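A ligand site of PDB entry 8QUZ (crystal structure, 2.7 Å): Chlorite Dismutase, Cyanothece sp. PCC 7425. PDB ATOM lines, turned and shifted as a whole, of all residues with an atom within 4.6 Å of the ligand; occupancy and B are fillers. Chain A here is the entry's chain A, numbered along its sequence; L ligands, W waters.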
ATOM      1  N   ASN A  64      -2.821  40.332  16.299  1.00  0.00           N
ATOM      2  CA  ASN A  64      -2.134  39.486  17.259  1.00  0.00           C
ATOM      3  C   ASN A  64      -2.452  37.998  17.031  1.00  0.00           C
ATOM      4  O   ASN A  64      -3.453  37.600  16.432  1.00  0.00           O
ATOM      5  CB  ASN A  64      -2.539  39.901  18.664  1.00  0.00           C
ATOM      6  CG  ASN A  64      -4.044  39.817  18.877  1.00  0.00           C
ATOM      7  OD1 ASN A  64      -4.799  40.670  18.400  1.00  0.00           O
ATOM      8  ND2 ASN A  64      -4.492  38.786  19.595  1.00  0.00           N
ATOM      9  N   ILE A  65      -1.584  37.169  17.616  1.00  0.00           N
ATOM     10  CA  ILE A  65      -1.691  35.720  17.541  1.00  0.00           C
ATOM     11  C   ILE A  65      -2.959  35.268  18.275  1.00  0.00           C
ATOM     12  O   ILE A  65      -3.228  35.734  19.376  1.00  0.00           O
ATOM     13  CB  ILE A  65      -0.400  35.130  18.138  1.00  0.00           C
ATOM     14  CG1 ILE A  65       0.765  35.264  17.158  1.00  0.00           C
ATOM     15  CG2 ILE A  65      -0.594  33.684  18.586  1.00  0.00           C
ATOM     16  CD1 ILE A  65       0.637  34.412  15.912  1.00  0.00           C
ATOM     17  N   ARG A  66      -3.721  34.354  17.652  1.00  0.00           N
ATOM     18  CA  ARG A  66      -4.948  33.832  18.246  1.00  0.00           C
ATOM     19  C   ARG A  66      -4.829  32.384  18.757  1.00  0.00           C
ATOM     20  O   ARG A  66      -5.610  32.022  19.656  1.00  0.00           O
ATOM     21  CB  ARG A  66      -6.105  33.928  17.233  1.00  0.00           C
ATOM     22  CG  ARG A  66      -6.197  35.256  16.497  1.00  0.00           C
ATOM     23  CD  ARG A  66      -6.403  36.458  17.409  1.00  0.00           C
ATOM     24  NE  ARG A  66      -6.660  37.714  16.705  1.00  0.00           N
ATOM     25  CZ  ARG A  66      -7.844  38.128  16.241  1.00  0.00           C
ATOM     26  NH1 ARG A  66      -8.959  37.455  16.488  1.00  0.00           N
ATOM     27  NH2 ARG A  66      -7.898  39.266  15.559  1.00  0.00           N
ATOM     28  N   TYR A  67      -3.917  31.542  18.223  1.00  0.00           N
ATOM     29  CA  TYR A  67      -3.915  30.111  18.578  1.00  0.00           C
ATOM     30  C   TYR A  67      -2.508  29.580  18.947  1.00  0.00           C
ATOM     31  O   TYR A  67      -2.367  28.766  19.873  1.00  0.00           O
ATOM     32  CB  TYR A  67      -4.514  29.259  17.453  1.00  0.00           C
ATOM     33  CG  TYR A  67      -5.977  29.511  17.182  1.00  0.00           C
ATOM     34  CD1 TYR A  67      -6.966  29.096  18.071  1.00  0.00           C
ATOM     35  CD2 TYR A  67      -6.383  30.242  16.064  1.00  0.00           C
ATOM     36  CE1 TYR A  67      -8.310  29.346  17.830  1.00  0.00           C
ATOM     37  CE2 TYR A  67      -7.723  30.521  15.828  1.00  0.00           C
ATOM     38  CZ  TYR A  67      -8.693  30.076  16.718  1.00  0.00           C
ATOM     39  OH  TYR A  67     -10.008  30.380  16.450  1.00  0.00           O
ATOM     40  N   ALA A  68      -1.473  30.021  18.219  1.00  0.00           N
ATOM     41  CA  ALA A  68      -0.119  29.529  18.434  1.00  0.00           C
ATOM     42  C   ALA A  68       0.376  29.729  19.870  1.00  0.00           C
ATOM     43  O   ALA A  68       0.258  30.792  20.465  1.00  0.00           O
ATOM     44  CB  ALA A  68       0.779  30.250  17.466  1.00  0.00           C
ATOM     45  N   LEU A  76       8.330  28.411  14.391  1.00  0.00           N
ATOM     46  CA  LEU A  76       8.045  29.220  13.216  1.00  0.00           C
ATOM     47  C   LEU A  76       9.161  30.227  12.978  1.00  0.00           C
ATOM     48  O   LEU A  76       9.594  30.403  11.850  1.00  0.00           O
ATOM     49  CB  LEU A  76       6.678  29.906  13.382  1.00  0.00           C
ATOM     50  CG  LEU A  76       5.496  28.925  13.379  1.00  0.00           C
ATOM     51  CD1 LEU A  76       4.276  29.531  14.034  1.00  0.00           C
ATOM     52  CD2 LEU A  76       5.174  28.459  11.965  1.00  0.00           C
ATOM     53  N   ILE A  94      -5.526  33.583  -0.906  1.00  0.00           N
ATOM     54  CA  ILE A  94      -6.588  32.625  -0.660  1.00  0.00           C
ATOM     55  C   ILE A  94      -7.511  33.172   0.421  1.00  0.00           C
ATOM     56  O   ILE A  94      -7.209  33.018   1.605  1.00  0.00           O
ATOM     57  CB  ILE A  94      -6.086  31.214  -0.301  1.00  0.00           C
ATOM     58  CG1 ILE A  94      -5.057  30.699  -1.296  1.00  0.00           C
ATOM     59  CG2 ILE A  94      -7.264  30.240  -0.167  1.00  0.00           C
ATOM     60  CD1 ILE A  94      -4.452  29.374  -0.918  1.00  0.00           C
ATOM     61  N   ILE A  96     -10.795  32.990   2.754  1.00  0.00           N
ATOM     62  CA  ILE A  96     -11.458  31.897   3.432  1.00  0.00           C
ATOM     63  C   ILE A  96     -12.547  32.483   4.322  1.00  0.00           C
ATOM     64  O   ILE A  96     -12.308  33.451   5.042  1.00  0.00           O
ATOM     65  CB  ILE A  96     -10.434  31.109   4.275  1.00  0.00           C
ATOM     66  CG1 ILE A  96      -9.539  30.254   3.382  1.00  0.00           C
ATOM     67  CG2 ILE A  96     -11.134  30.265   5.332  1.00  0.00           C
ATOM     68  CD1 ILE A  96      -8.229  29.919   4.009  1.00  0.00           C
ATOM     69  N   LYS A  98     -15.162  30.869   7.359  1.00  0.00           N
ATOM     70  CA  LYS A  98     -15.549  29.739   8.195  1.00  0.00           C
ATOM     71  C   LYS A  98     -17.005  29.882   8.623  1.00  0.00           C
ATOM     72  O   LYS A  98     -17.576  30.961   8.510  1.00  0.00           O
ATOM     73  CB  LYS A  98     -14.595  29.687   9.389  1.00  0.00           C
ATOM     74  CG  LYS A  98     -13.164  29.327   9.044  1.00  0.00           C
ATOM     75  CD  LYS A  98     -12.375  28.865  10.237  1.00  0.00           C
ATOM     76  CE  LYS A  98     -10.934  28.519   9.907  1.00  0.00           C
ATOM     77  NZ  LYS A  98     -10.107  28.204  11.110  1.00  0.00           N
ATOM     78  N   TRP A 102     -18.439  27.393  13.597  1.00  0.00           N
ATOM     79  CA  TRP A 102     -17.057  27.622  14.019  1.00  0.00           C
ATOM     80  C   TRP A 102     -16.991  28.816  14.951  1.00  0.00           C
ATOM     81  O   TRP A 102     -16.433  28.708  16.039  1.00  0.00           O
ATOM     82  CB  TRP A 102     -16.130  27.825  12.818  1.00  0.00           C
ATOM     83  CG  TRP A 102     -14.736  28.263  13.191  1.00  0.00           C
ATOM     84  CD1 TRP A 102     -14.229  29.536  13.162  1.00  0.00           C
ATOM     85  CD2 TRP A 102     -13.633  27.420  13.621  1.00  0.00           C
ATOM     86  NE1 TRP A 102     -12.932  29.545  13.581  1.00  0.00           N
ATOM     87  CE2 TRP A 102     -12.539  28.263  13.852  1.00  0.00           C
ATOM     88  CE3 TRP A 102     -13.487  26.047  13.825  1.00  0.00           C
ATOM     89  CZ2 TRP A 102     -11.298  27.784  14.268  1.00  0.00           C
ATOM     90  CZ3 TRP A 102     -12.267  25.560  14.241  1.00  0.00           C
ATOM     91  CH2 TRP A 102     -11.179  26.420  14.461  1.00  0.00           C
ATOM     92  N   PHE A 114      -8.016  23.125  15.575  1.00  0.00           N
ATOM     93  CA  PHE A 114      -6.982  23.761  14.765  1.00  0.00           C
ATOM     94  C   PHE A 114      -5.654  22.999  14.856  1.00  0.00           C
ATOM     95  O   PHE A 114      -5.010  22.759  13.827  1.00  0.00           O
ATOM     96  CB  PHE A 114      -6.851  25.233  15.173  1.00  0.00           C
ATOM     97  CG  PHE A 114      -5.747  25.986  14.479  1.00  0.00           C
ATOM     98  CD1 PHE A 114      -5.922  26.499  13.206  1.00  0.00           C
ATOM     99  CD2 PHE A 114      -4.511  26.147  15.096  1.00  0.00           C
ATOM    100  CE1 PHE A 114      -4.896  27.164  12.553  1.00  0.00           C
ATOM    101  CE2 PHE A 114      -3.480  26.809  14.435  1.00  0.00           C
ATOM    102  CZ  PHE A 114      -3.673  27.307  13.167  1.00  0.00           C
ATOM    103  N   HIS A 120      -2.473  22.023  12.100  1.00  0.00           N
ATOM    104  CA  HIS A 120      -2.290  23.107  11.133  1.00  0.00           C
ATOM    105  C   HIS A 120      -0.833  23.590  11.119  1.00  0.00           C
ATOM    106  O   HIS A 120      -0.231  23.712  10.068  1.00  0.00           O
ATOM    107  CB  HIS A 120      -3.278  24.247  11.388  1.00  0.00           C
ATOM    108  CG  HIS A 120      -3.220  25.367  10.386  1.00  0.00           C
ATOM    109  ND1 HIS A 120      -4.307  25.669   9.601  1.00  0.00           N
ATOM    110  CD2 HIS A 120      -2.266  26.272  10.061  1.00  0.00           C
ATOM    111  CE1 HIS A 120      -4.000  26.699   8.824  1.00  0.00           C
ATOM    112  NE2 HIS A 120      -2.761  27.074   9.071  1.00  0.00           N
ATOM    113  N   THR A 121      -0.267  23.845  12.292  1.00  0.00           N
ATOM    114  CA  THR A 121       1.067  24.415  12.372  1.00  0.00           C
ATOM    115  C   THR A 121       2.130  23.361  12.061  1.00  0.00           C
ATOM    116  O   THR A 121       3.031  23.617  11.276  1.00  0.00           O
ATOM    117  CB  THR A 121       1.268  25.065  13.747  1.00  0.00           C
ATOM    118  OG1 THR A 121       0.203  25.965  14.039  1.00  0.00           O
ATOM    119  CG2 THR A 121       2.560  25.839  13.816  1.00  0.00           C
ATOM    120  N   GLY A 124       2.018  22.798   8.318  1.00  0.00           N
ATOM    121  CA  GLY A 124       2.502  23.959   7.588  1.00  0.00           C
ATOM    122  C   GLY A 124       4.006  24.125   7.677  1.00  0.00           C
ATOM    123  O   GLY A 124       4.632  24.527   6.691  1.00  0.00           O
ATOM    124  N   LEU A 125       4.567  23.814   8.853  1.00  0.00           N
ATOM    125  CA  LEU A 125       6.016  23.845   9.102  1.00  0.00           C
ATOM    126  C   LEU A 125       6.805  22.945   8.141  1.00  0.00           C
ATOM    127  O   LEU A 125       7.974  23.192   7.873  1.00  0.00           O
ATOM    128  CB  LEU A 125       6.286  23.431  10.545  1.00  0.00           C
ATOM    129  CG  LEU A 125       6.580  24.581  11.503  1.00  0.00           C
ATOM    130  CD1 LEU A 125       6.749  24.065  12.921  1.00  0.00           C
ATOM    131  CD2 LEU A 125       7.824  25.343  11.066  1.00  0.00           C
ATOM    132  N   LEU A 128       8.097  25.031   5.085  1.00  0.00           N
ATOM    133  CA  LEU A 128       8.996  26.159   5.311  1.00  0.00           C
ATOM    134  C   LEU A 128      10.423  25.650   5.227  1.00  0.00           C
ATOM    135  O   LEU A 128      10.629  24.503   5.602  1.00  0.00           O
ATOM    136  CB  LEU A 128       8.691  26.726   6.704  1.00  0.00           C
ATOM    137  CG  LEU A 128       7.751  27.919   6.719  1.00  0.00           C
ATOM    138  CD1 LEU A 128       6.525  27.646   5.900  1.00  0.00           C
ATOM    139  CD2 LEU A 128       7.374  28.281   8.141  1.00  0.00           C
ATOM    140  N   VAL A 131       8.010  28.284   1.470  1.00  0.00           N
ATOM    141  CA  VAL A 131       6.819  29.153   1.431  1.00  0.00           C
ATOM    142  C   VAL A 131       6.869  30.269   2.476  1.00  0.00           C
ATOM    143  O   VAL A 131       6.918  30.022   3.685  1.00  0.00           O
ATOM    144  CB  VAL A 131       5.529  28.334   1.625  1.00  0.00           C
ATOM    145  CG1 VAL A 131       4.311  29.246   1.533  1.00  0.00           C
ATOM    146  CG2 VAL A 131       5.408  27.178   0.647  1.00  0.00           C
ATOM    147  N   ARG A 133       4.471  33.521   4.035  1.00  0.00           N
ATOM    148  CA  ARG A 133       3.037  33.692   4.254  1.00  0.00           C
ATOM    149  C   ARG A 133       2.720  35.003   4.977  1.00  0.00           C
ATOM    150  O   ARG A 133       3.533  35.539   5.704  1.00  0.00           O
ATOM    151  CB  ARG A 133       2.475  32.498   5.028  1.00  0.00           C
ATOM    152  CG  ARG A 133       2.876  32.463   6.500  1.00  0.00           C
ATOM    153  CD  ARG A 133       2.523  31.150   7.182  1.00  0.00           C
ATOM    154  NE  ARG A 133       2.581  31.285   8.631  1.00  0.00           N
ATOM    155  CZ  ARG A 133       3.695  31.368   9.357  1.00  0.00           C
ATOM    156  NH1 ARG A 133       4.885  31.181   8.814  1.00  0.00           N
ATOM    157  NH2 ARG A 133       3.632  31.628  10.643  1.00  0.00           N
ATOM    158  N   LEU A 135      -0.906  36.606   7.085  1.00  0.00           N
ATOM    159  CA  LEU A 135      -2.281  36.358   7.472  1.00  0.00           C
ATOM    160  C   LEU A 135      -2.963  37.659   7.865  1.00  0.00           C
ATOM    161  O   LEU A 135      -2.459  38.435   8.689  1.00  0.00           O
ATOM    162  CB  LEU A 135      -2.319  35.363   8.627  1.00  0.00           C
ATOM    163  CG  LEU A 135      -3.694  35.157   9.239  1.00  0.00           C
ATOM    164  CD1 LEU A 135      -4.648  34.536   8.258  1.00  0.00           C
ATOM    165  CD2 LEU A 135      -3.610  34.295  10.490  1.00  0.00           C
ATOM    166  N   HIS A 137      -6.967  39.307   8.854  1.00  0.00           N
ATOM    167  CA  HIS A 137      -8.285  39.074   9.416  1.00  0.00           C
ATOM    168  C   HIS A 137      -9.267  40.095   8.820  1.00  0.00           C
ATOM    169  O   HIS A 137      -8.862  41.260   8.646  1.00  0.00           O
ATOM    170  CB  HIS A 137      -8.203  39.261  10.929  1.00  0.00           C
ATOM    171  CG  HIS A 137      -7.249  38.341  11.595  1.00  0.00           C
ATOM    172  ND1 HIS A 137      -7.661  37.221  12.312  1.00  0.00           N
ATOM    173  CD2 HIS A 137      -5.899  38.356  11.650  1.00  0.00           C
ATOM    174  CE1 HIS A 137      -6.584  36.612  12.785  1.00  0.00           C
ATOM    175  NE2 HIS A 137      -5.508  37.281  12.386  1.00  0.00           N
ATOM    176  N   PHE A 147     -11.025  35.730   6.257  1.00  0.00           N
ATOM    177  CA  PHE A 147      -9.570  35.841   6.235  1.00  0.00           C
ATOM    178  C   PHE A 147      -9.040  35.999   4.814  1.00  0.00           C
ATOM    179  O   PHE A 147      -9.615  35.486   3.876  1.00  0.00           O
ATOM    180  CB  PHE A 147      -8.852  34.601   6.791  1.00  0.00           C
ATOM    181  CG  PHE A 147      -9.302  34.109   8.145  1.00  0.00           C
ATOM    182  CD1 PHE A 147      -8.902  34.744   9.309  1.00  0.00           C
ATOM    183  CD2 PHE A 147     -10.152  33.026   8.251  1.00  0.00           C
ATOM    184  CE1 PHE A 147      -9.336  34.294  10.551  1.00  0.00           C
ATOM    185  CE2 PHE A 147     -10.589  32.583   9.488  1.00  0.00           C
ATOM    186  CZ  PHE A 147     -10.195  33.226  10.630  1.00  0.00           C
ATOM    187  N   THR A 149      -5.395  35.037   3.114  1.00  0.00           N
ATOM    188  CA  THR A 149      -4.118  34.409   3.351  1.00  0.00           C
ATOM    189  C   THR A 149      -3.279  34.649   2.118  1.00  0.00           C
ATOM    190  O   THR A 149      -3.801  34.751   1.021  1.00  0.00           O
ATOM    191  CB  THR A 149      -4.283  32.928   3.715  1.00  0.00           C
ATOM    192  OG1 THR A 149      -4.784  32.185   2.610  1.00  0.00           O
ATOM    193  CG2 THR A 149      -5.203  32.758   4.908  1.00  0.00           C
ATOM    194  N   PHE A 151       0.585  33.719   0.284  1.00  0.00           N
ATOM    195  CA  PHE A 151       1.705  32.800   0.193  1.00  0.00           C
ATOM    196  C   PHE A 151       2.539  33.150  -1.024  1.00  0.00           C
ATOM    197  O   PHE A 151       1.974  33.385  -2.089  1.00  0.00           O
ATOM    198  CB  PHE A 151       1.242  31.346   0.048  1.00  0.00           C
ATOM    199  CG  PHE A 151       0.232  30.979   1.090  1.00  0.00           C
ATOM    200  CD1 PHE A 151       0.645  30.627   2.352  1.00  0.00           C
ATOM    201  CD2 PHE A 151      -1.114  31.154   0.851  1.00  0.00           C
ATOM    202  CE1 PHE A 151      -0.279  30.344   3.346  1.00  0.00           C
ATOM    203  CE2 PHE A 151      -2.043  30.912   1.851  1.00  0.00           C
ATOM    204  CZ  PHE A 151      -1.626  30.495   3.090  1.00  0.00           C
ATOM    205  N   PHE A 161       3.585  23.376  -2.676  1.00  0.00           N
ATOM    206  CA  PHE A 161       2.488  24.224  -2.225  1.00  0.00           C
ATOM    207  C   PHE A 161       1.152  23.550  -2.547  1.00  0.00           C
ATOM    208  O   PHE A 161       0.248  23.554  -1.697  1.00  0.00           O
ATOM    209  CB  PHE A 161       2.560  25.645  -2.814  1.00  0.00           C
ATOM    210  CG  PHE A 161       1.498  26.562  -2.244  1.00  0.00           C
ATOM    211  CD1 PHE A 161       1.580  27.013  -0.935  1.00  0.00           C
ATOM    212  CD2 PHE A 161       0.357  26.867  -2.979  1.00  0.00           C
ATOM    213  CE1 PHE A 161       0.555  27.771  -0.375  1.00  0.00           C
ATOM    214  CE2 PHE A 161      -0.653  27.648  -2.430  1.00  0.00           C
ATOM    215  CZ  PHE A 161      -0.548  28.091  -1.127  1.00  0.00           C
ATOM    216  N   LEU A 164       0.513  20.901  -0.079  1.00  0.00           N
ATOM    217  CA  LEU A 164       0.046  21.504   1.170  1.00  0.00           C
ATOM    218  C   LEU A 164      -1.455  21.842   1.116  1.00  0.00           C
ATOM    219  O   LEU A 164      -2.188  21.503   2.044  1.00  0.00           O
ATOM    220  CB  LEU A 164       0.924  22.700   1.525  1.00  0.00           C
ATOM    221  CG  LEU A 164       0.395  23.634   2.627  1.00  0.00           C
ATOM    222  CD1 LEU A 164       0.400  22.953   3.995  1.00  0.00           C
ATOM    223  CD2 LEU A 164       1.200  24.919   2.670  1.00  0.00           C
ATOM    224  N   LEU A 165      -1.955  22.459   0.025  1.00  0.00           N
ATOM    225  CA  LEU A 165      -3.359  22.833  -0.061  1.00  0.00           C
ATOM    226  C   LEU A 165      -4.252  21.625   0.143  1.00  0.00           C
ATOM    227  O   LEU A 165      -5.292  21.731   0.787  1.00  0.00           O
ATOM    228  CB  LEU A 165      -3.673  23.408  -1.431  1.00  0.00           C
ATOM    229  CG  LEU A 165      -3.187  24.835  -1.703  1.00  0.00           C
ATOM    230  CD1 LEU A 165      -3.494  25.194  -3.153  1.00  0.00           C
ATOM    231  CD2 LEU A 165      -3.817  25.863  -0.763  1.00  0.00           C
ATOM    232  N   MET A 168      -4.381  20.404   3.829  1.00  0.00           N
ATOM    233  CA  MET A 168      -5.145  21.250   4.737  1.00  0.00           C
ATOM    234  C   MET A 168      -6.632  20.973   4.533  1.00  0.00           C
ATOM    235  O   MET A 168      -7.383  20.858   5.502  1.00  0.00           O
ATOM    236  CB  MET A 168      -4.856  22.725   4.448  1.00  0.00           C
ATOM    237  CG  MET A 168      -3.458  23.204   4.861  1.00  0.00           C
ATOM    238  SD  MET A 168      -3.269  23.285   6.640  1.00  0.00           S
ATOM    239  CE  MET A 168      -1.857  24.373   6.796  1.00  0.00           C
ATOM    240  N   GLU A 173     -10.337  20.851  10.524  1.00  0.00           N
ATOM    241  CA  GLU A 173     -10.514  22.292  10.415  1.00  0.00           C
ATOM    242  C   GLU A 173     -11.341  22.650   9.182  1.00  0.00           C
ATOM    243  O   GLU A 173     -12.230  23.490   9.263  1.00  0.00           O
ATOM    244  CB  GLU A 173      -9.158  23.012  10.356  1.00  0.00           C
ATOM    245  CG  GLU A 173      -9.257  24.532  10.452  1.00  0.00           C
ATOM    246  CD  GLU A 173      -7.944  25.283  10.331  1.00  0.00           C
ATOM    247  OE1 GLU A 173      -6.917  24.624  10.096  1.00  0.00           O
ATOM    248  OE2 GLU A 173      -7.933  26.555  10.470  1.00  0.00           O
ATOM    249  N   TRP A 174     -11.032  22.034   8.027  1.00  0.00           N
ATOM    250  CA  TRP A 174     -11.587  22.492   6.769  1.00  0.00           C
ATOM    251  C   TRP A 174     -13.054  22.118   6.580  1.00  0.00           C
ATOM    252  O   TRP A 174     -13.660  22.572   5.633  1.00  0.00           O
ATOM    253  CB  TRP A 174     -10.762  22.056   5.549  1.00  0.00           C
ATOM    254  CG  TRP A 174     -10.185  23.235   4.819  1.00  0.00           C
ATOM    255  CD1 TRP A 174     -10.625  23.743   3.632  1.00  0.00           C
ATOM    256  CD2 TRP A 174      -9.076  24.079   5.225  1.00  0.00           C
ATOM    257  NE1 TRP A 174      -9.872  24.832   3.270  1.00  0.00           N
ATOM    258  CE2 TRP A 174      -8.908  25.058   4.222  1.00  0.00           C
ATOM    259  CE3 TRP A 174      -8.188  24.084   6.315  1.00  0.00           C
ATOM    260  CZ2 TRP A 174      -7.914  26.034   4.291  1.00  0.00           C
ATOM    261  CZ3 TRP A 174      -7.191  25.035   6.383  1.00  0.00           C
ATOM    262  CH2 TRP A 174      -7.066  26.016   5.386  1.00  0.00           C
ATOM    263  N   GLU A 180     -14.130  29.553  -0.305  1.00  0.00           N
ATOM    264  CA  GLU A 180     -12.700  29.531  -0.562  1.00  0.00           C
ATOM    265  C   GLU A 180     -12.463  29.813  -2.042  1.00  0.00           C
ATOM    266  O   GLU A 180     -13.219  29.325  -2.892  1.00  0.00           O
ATOM    267  CB  GLU A 180     -12.131  28.183  -0.162  1.00  0.00           C
ATOM    268  CG  GLU A 180     -10.630  28.100  -0.269  1.00  0.00           C
ATOM    269  CD  GLU A 180     -10.052  26.825   0.323  1.00  0.00           C
ATOM    270  OE1 GLU A 180     -10.852  25.945   0.829  1.00  0.00           O
ATOM    271  OE2 GLU A 180      -8.787  26.708   0.283  1.00  0.00           O
HETATM  272  C1  LIG L   1      -3.620  30.495  10.853  1.00  0.00           C
HETATM  273  C2  LIG L   1       0.739  28.646  10.112  1.00  0.00           C
HETATM  274  C3  LIG L   1      -0.434  27.542   5.593  1.00  0.00           C
HETATM  275  C4  LIG L   1      -4.902  29.088   6.440  1.00  0.00           C
HETATM  276  C5  LIG L   1      -2.343  30.034  11.021  1.00  0.00           C
HETATM  277  C6  LIG L   1      -1.671  30.078  12.273  1.00  0.00           C
HETATM  278  C7  LIG L   1      -0.436  29.570  12.047  1.00  0.00           C
HETATM  279  C8  LIG L   1      -0.356  29.211  10.682  1.00  0.00           C
HETATM  280  C9  LIG L   1       0.652  29.372  13.073  1.00  0.00           C
HETATM  281  C10 LIG L   1      -2.191  30.571  13.591  1.00  0.00           C
HETATM  282  C11 LIG L   1      -2.094  32.084  13.727  1.00  0.00           C
HETATM  283  C12 LIG L   1      -2.547  32.575  15.100  1.00  0.00           C
HETATM  284  O1  LIG L   1      -3.114  33.677  15.129  1.00  0.00           O
HETATM  285  O2  LIG L   1      -2.395  31.934  16.179  1.00  0.00           O
HETATM  286  C13 LIG L   1       0.789  28.223   8.817  1.00  0.00           C
HETATM  287  C14 LIG L   1       1.976  27.747   8.257  1.00  0.00           C
HETATM  288  C15 LIG L   1       1.682  27.423   6.981  1.00  0.00           C
HETATM  289  C16 LIG L   1       0.274  27.745   6.766  1.00  0.00           C
HETATM  290  C17 LIG L   1       3.345  27.607   8.864  1.00  0.00           C
HETATM  291  C18 LIG L   1       2.736  27.006   6.060  1.00  0.00           C
HETATM  292  C19 LIG L   1       2.615  27.354   4.777  1.00  0.00           C
HETATM  293  C20 LIG L   1      -1.772  27.812   5.415  1.00  0.00           C
HETATM  294  C21 LIG L   1      -2.535  27.659   4.231  1.00  0.00           C
HETATM  295  C22 LIG L   1      -3.789  28.125   4.498  1.00  0.00           C
HETATM  296  C23 LIG L   1      -3.803  28.540   5.839  1.00  0.00           C
HETATM  297  C24 LIG L   1      -2.074  27.118   2.911  1.00  0.00           C
HETATM  298  C25 LIG L   1      -4.968  28.170   3.624  1.00  0.00           C
HETATM  299  C26 LIG L   1      -5.036  27.671   2.402  1.00  0.00           C
HETATM  300  C27 LIG L   1      -4.878  29.625   7.720  1.00  0.00           C
HETATM  301  C28 LIG L   1      -6.022  30.331   8.299  1.00  0.00           C
HETATM  302  C29 LIG L   1      -5.658  30.728   9.520  1.00  0.00           C
HETATM  303  C30 LIG L   1      -4.280  30.279   9.656  1.00  0.00           C
HETATM  304  C31 LIG L   1      -7.381  30.577   7.657  1.00  0.00           C
HETATM  305  C32 LIG L   1      -6.500  31.467  10.492  1.00  0.00           C
HETATM  306  C33 LIG L   1      -7.311  30.494  11.324  1.00  0.00           C
HETATM  307  C34 LIG L   1      -8.187  31.205  12.347  1.00  0.00           C
HETATM  308  O3  LIG L   1      -7.785  32.258  12.946  1.00  0.00           O
HETATM  309  O4  LIG L   1      -9.322  30.712  12.571  1.00  0.00           O
HETATM  310  N1  LIG L   1      -1.507  29.501  10.039  1.00  0.00           N
HETATM  311  N2  LIG L   1      -0.173  28.229   7.906  1.00  0.00           N
HETATM  312  N3  LIG L   1      -2.561  28.324   6.361  1.00  0.00           N
HETATM  313  N4  LIG L   1      -3.836  29.625   8.545  1.00  0.00           N
HETATM  314 FE1  LIG L   1      -2.101  28.870   8.245  1.00  0.00          FE
HETATM  315  O   HOH W   1      -1.013  31.544   7.641  1.00  0.00           O
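Merely in contact with the ligand: Ile 65 (3.5 Å), Leu 76 (3.7 Å), Ile 94 (3.8 Å), Ile 96 (3.7 Å), Trp 102 (3.9 Å), Phe 114 (3.5 Å), Thr 121 (3.6 Å), Gly 124 (3.2 Å), Leu 125 (3.99 Å), Leu 128 (3.8 Å), Arg 133 (3.5 Å), Leu 135 (3.8 Å), Phe 147 (3.3 Å), Thr 149 (3.99 Å), Phe 151 (3.2 Å), Leu 164 (3.5 Å), Leu 165 (3.8 Å), Met 168 (3.7 Å) and Trp 174 (3.5 Å).
24 residues have an atom within 4 Å of the ligand: Ile 65, Arg 66, Tyr 67, Ala 68, Leu 76, Ile 94, Ile 96, Lys 98, Trp 102, Phe 114, His 120, Thr 121, Gly 124, Leu 125, Leu 128, Arg 133, Leu 135, Phe 147, Thr 149, Phe 151, Leu 164, Leu 165, Met 168 and Trp 174.
The nearest printed residue that does not touch the ligand is Glu 173 (4.1 Å).
O of Ile 94 lies within hydrogen-bond range of OG1 of Thr 149 (2.8 Å).
The side-chain amino group (NZ) of Lys 98 lies within salt-bridge range of the side-chain carboxylate (OE2) of Glu 173, 2.8 Å away.
NE of Arg 66 lies within hydrogen-bond range of O of Asn 64.
The side-chain carboxylate (OE1) of Glu 180 is in hydrogen-bond range of the indole nitrogen (NE1) of Trp 174 (2.9 Å).
ND1 of His 120 lies within hydrogen-bond range of OE1 of Glu 173 (2.9 Å).
N of His 120 sits at hydrogen-bond distance from O of Phe 114 (3.2 Å).
The backbone carbonyl oxygen (O) of Ile 96 is in hydrogen-bond range of the backbone NH (N) of Phe 147 (2.9 Å).
N of Arg 66 is in hydrogen-bond range of O1 of the ligand, at 2.7 Å.
FE1 of the ligand is bound by NE2 of His 120 (2.1 Å).
An oxygen (O2) of the ligand is in hydrogen-bond range of the backbone NH (N) of Tyr 67 (2.6 Å).
O4 of the ligand lies within salt-bridge range of NZ of Lys 98, 3.0 Å away.
The backbone NH (N) of Ala 68 sits at hydrogen-bond distance from an oxygen (O2) of the ligand (2.9 Å).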
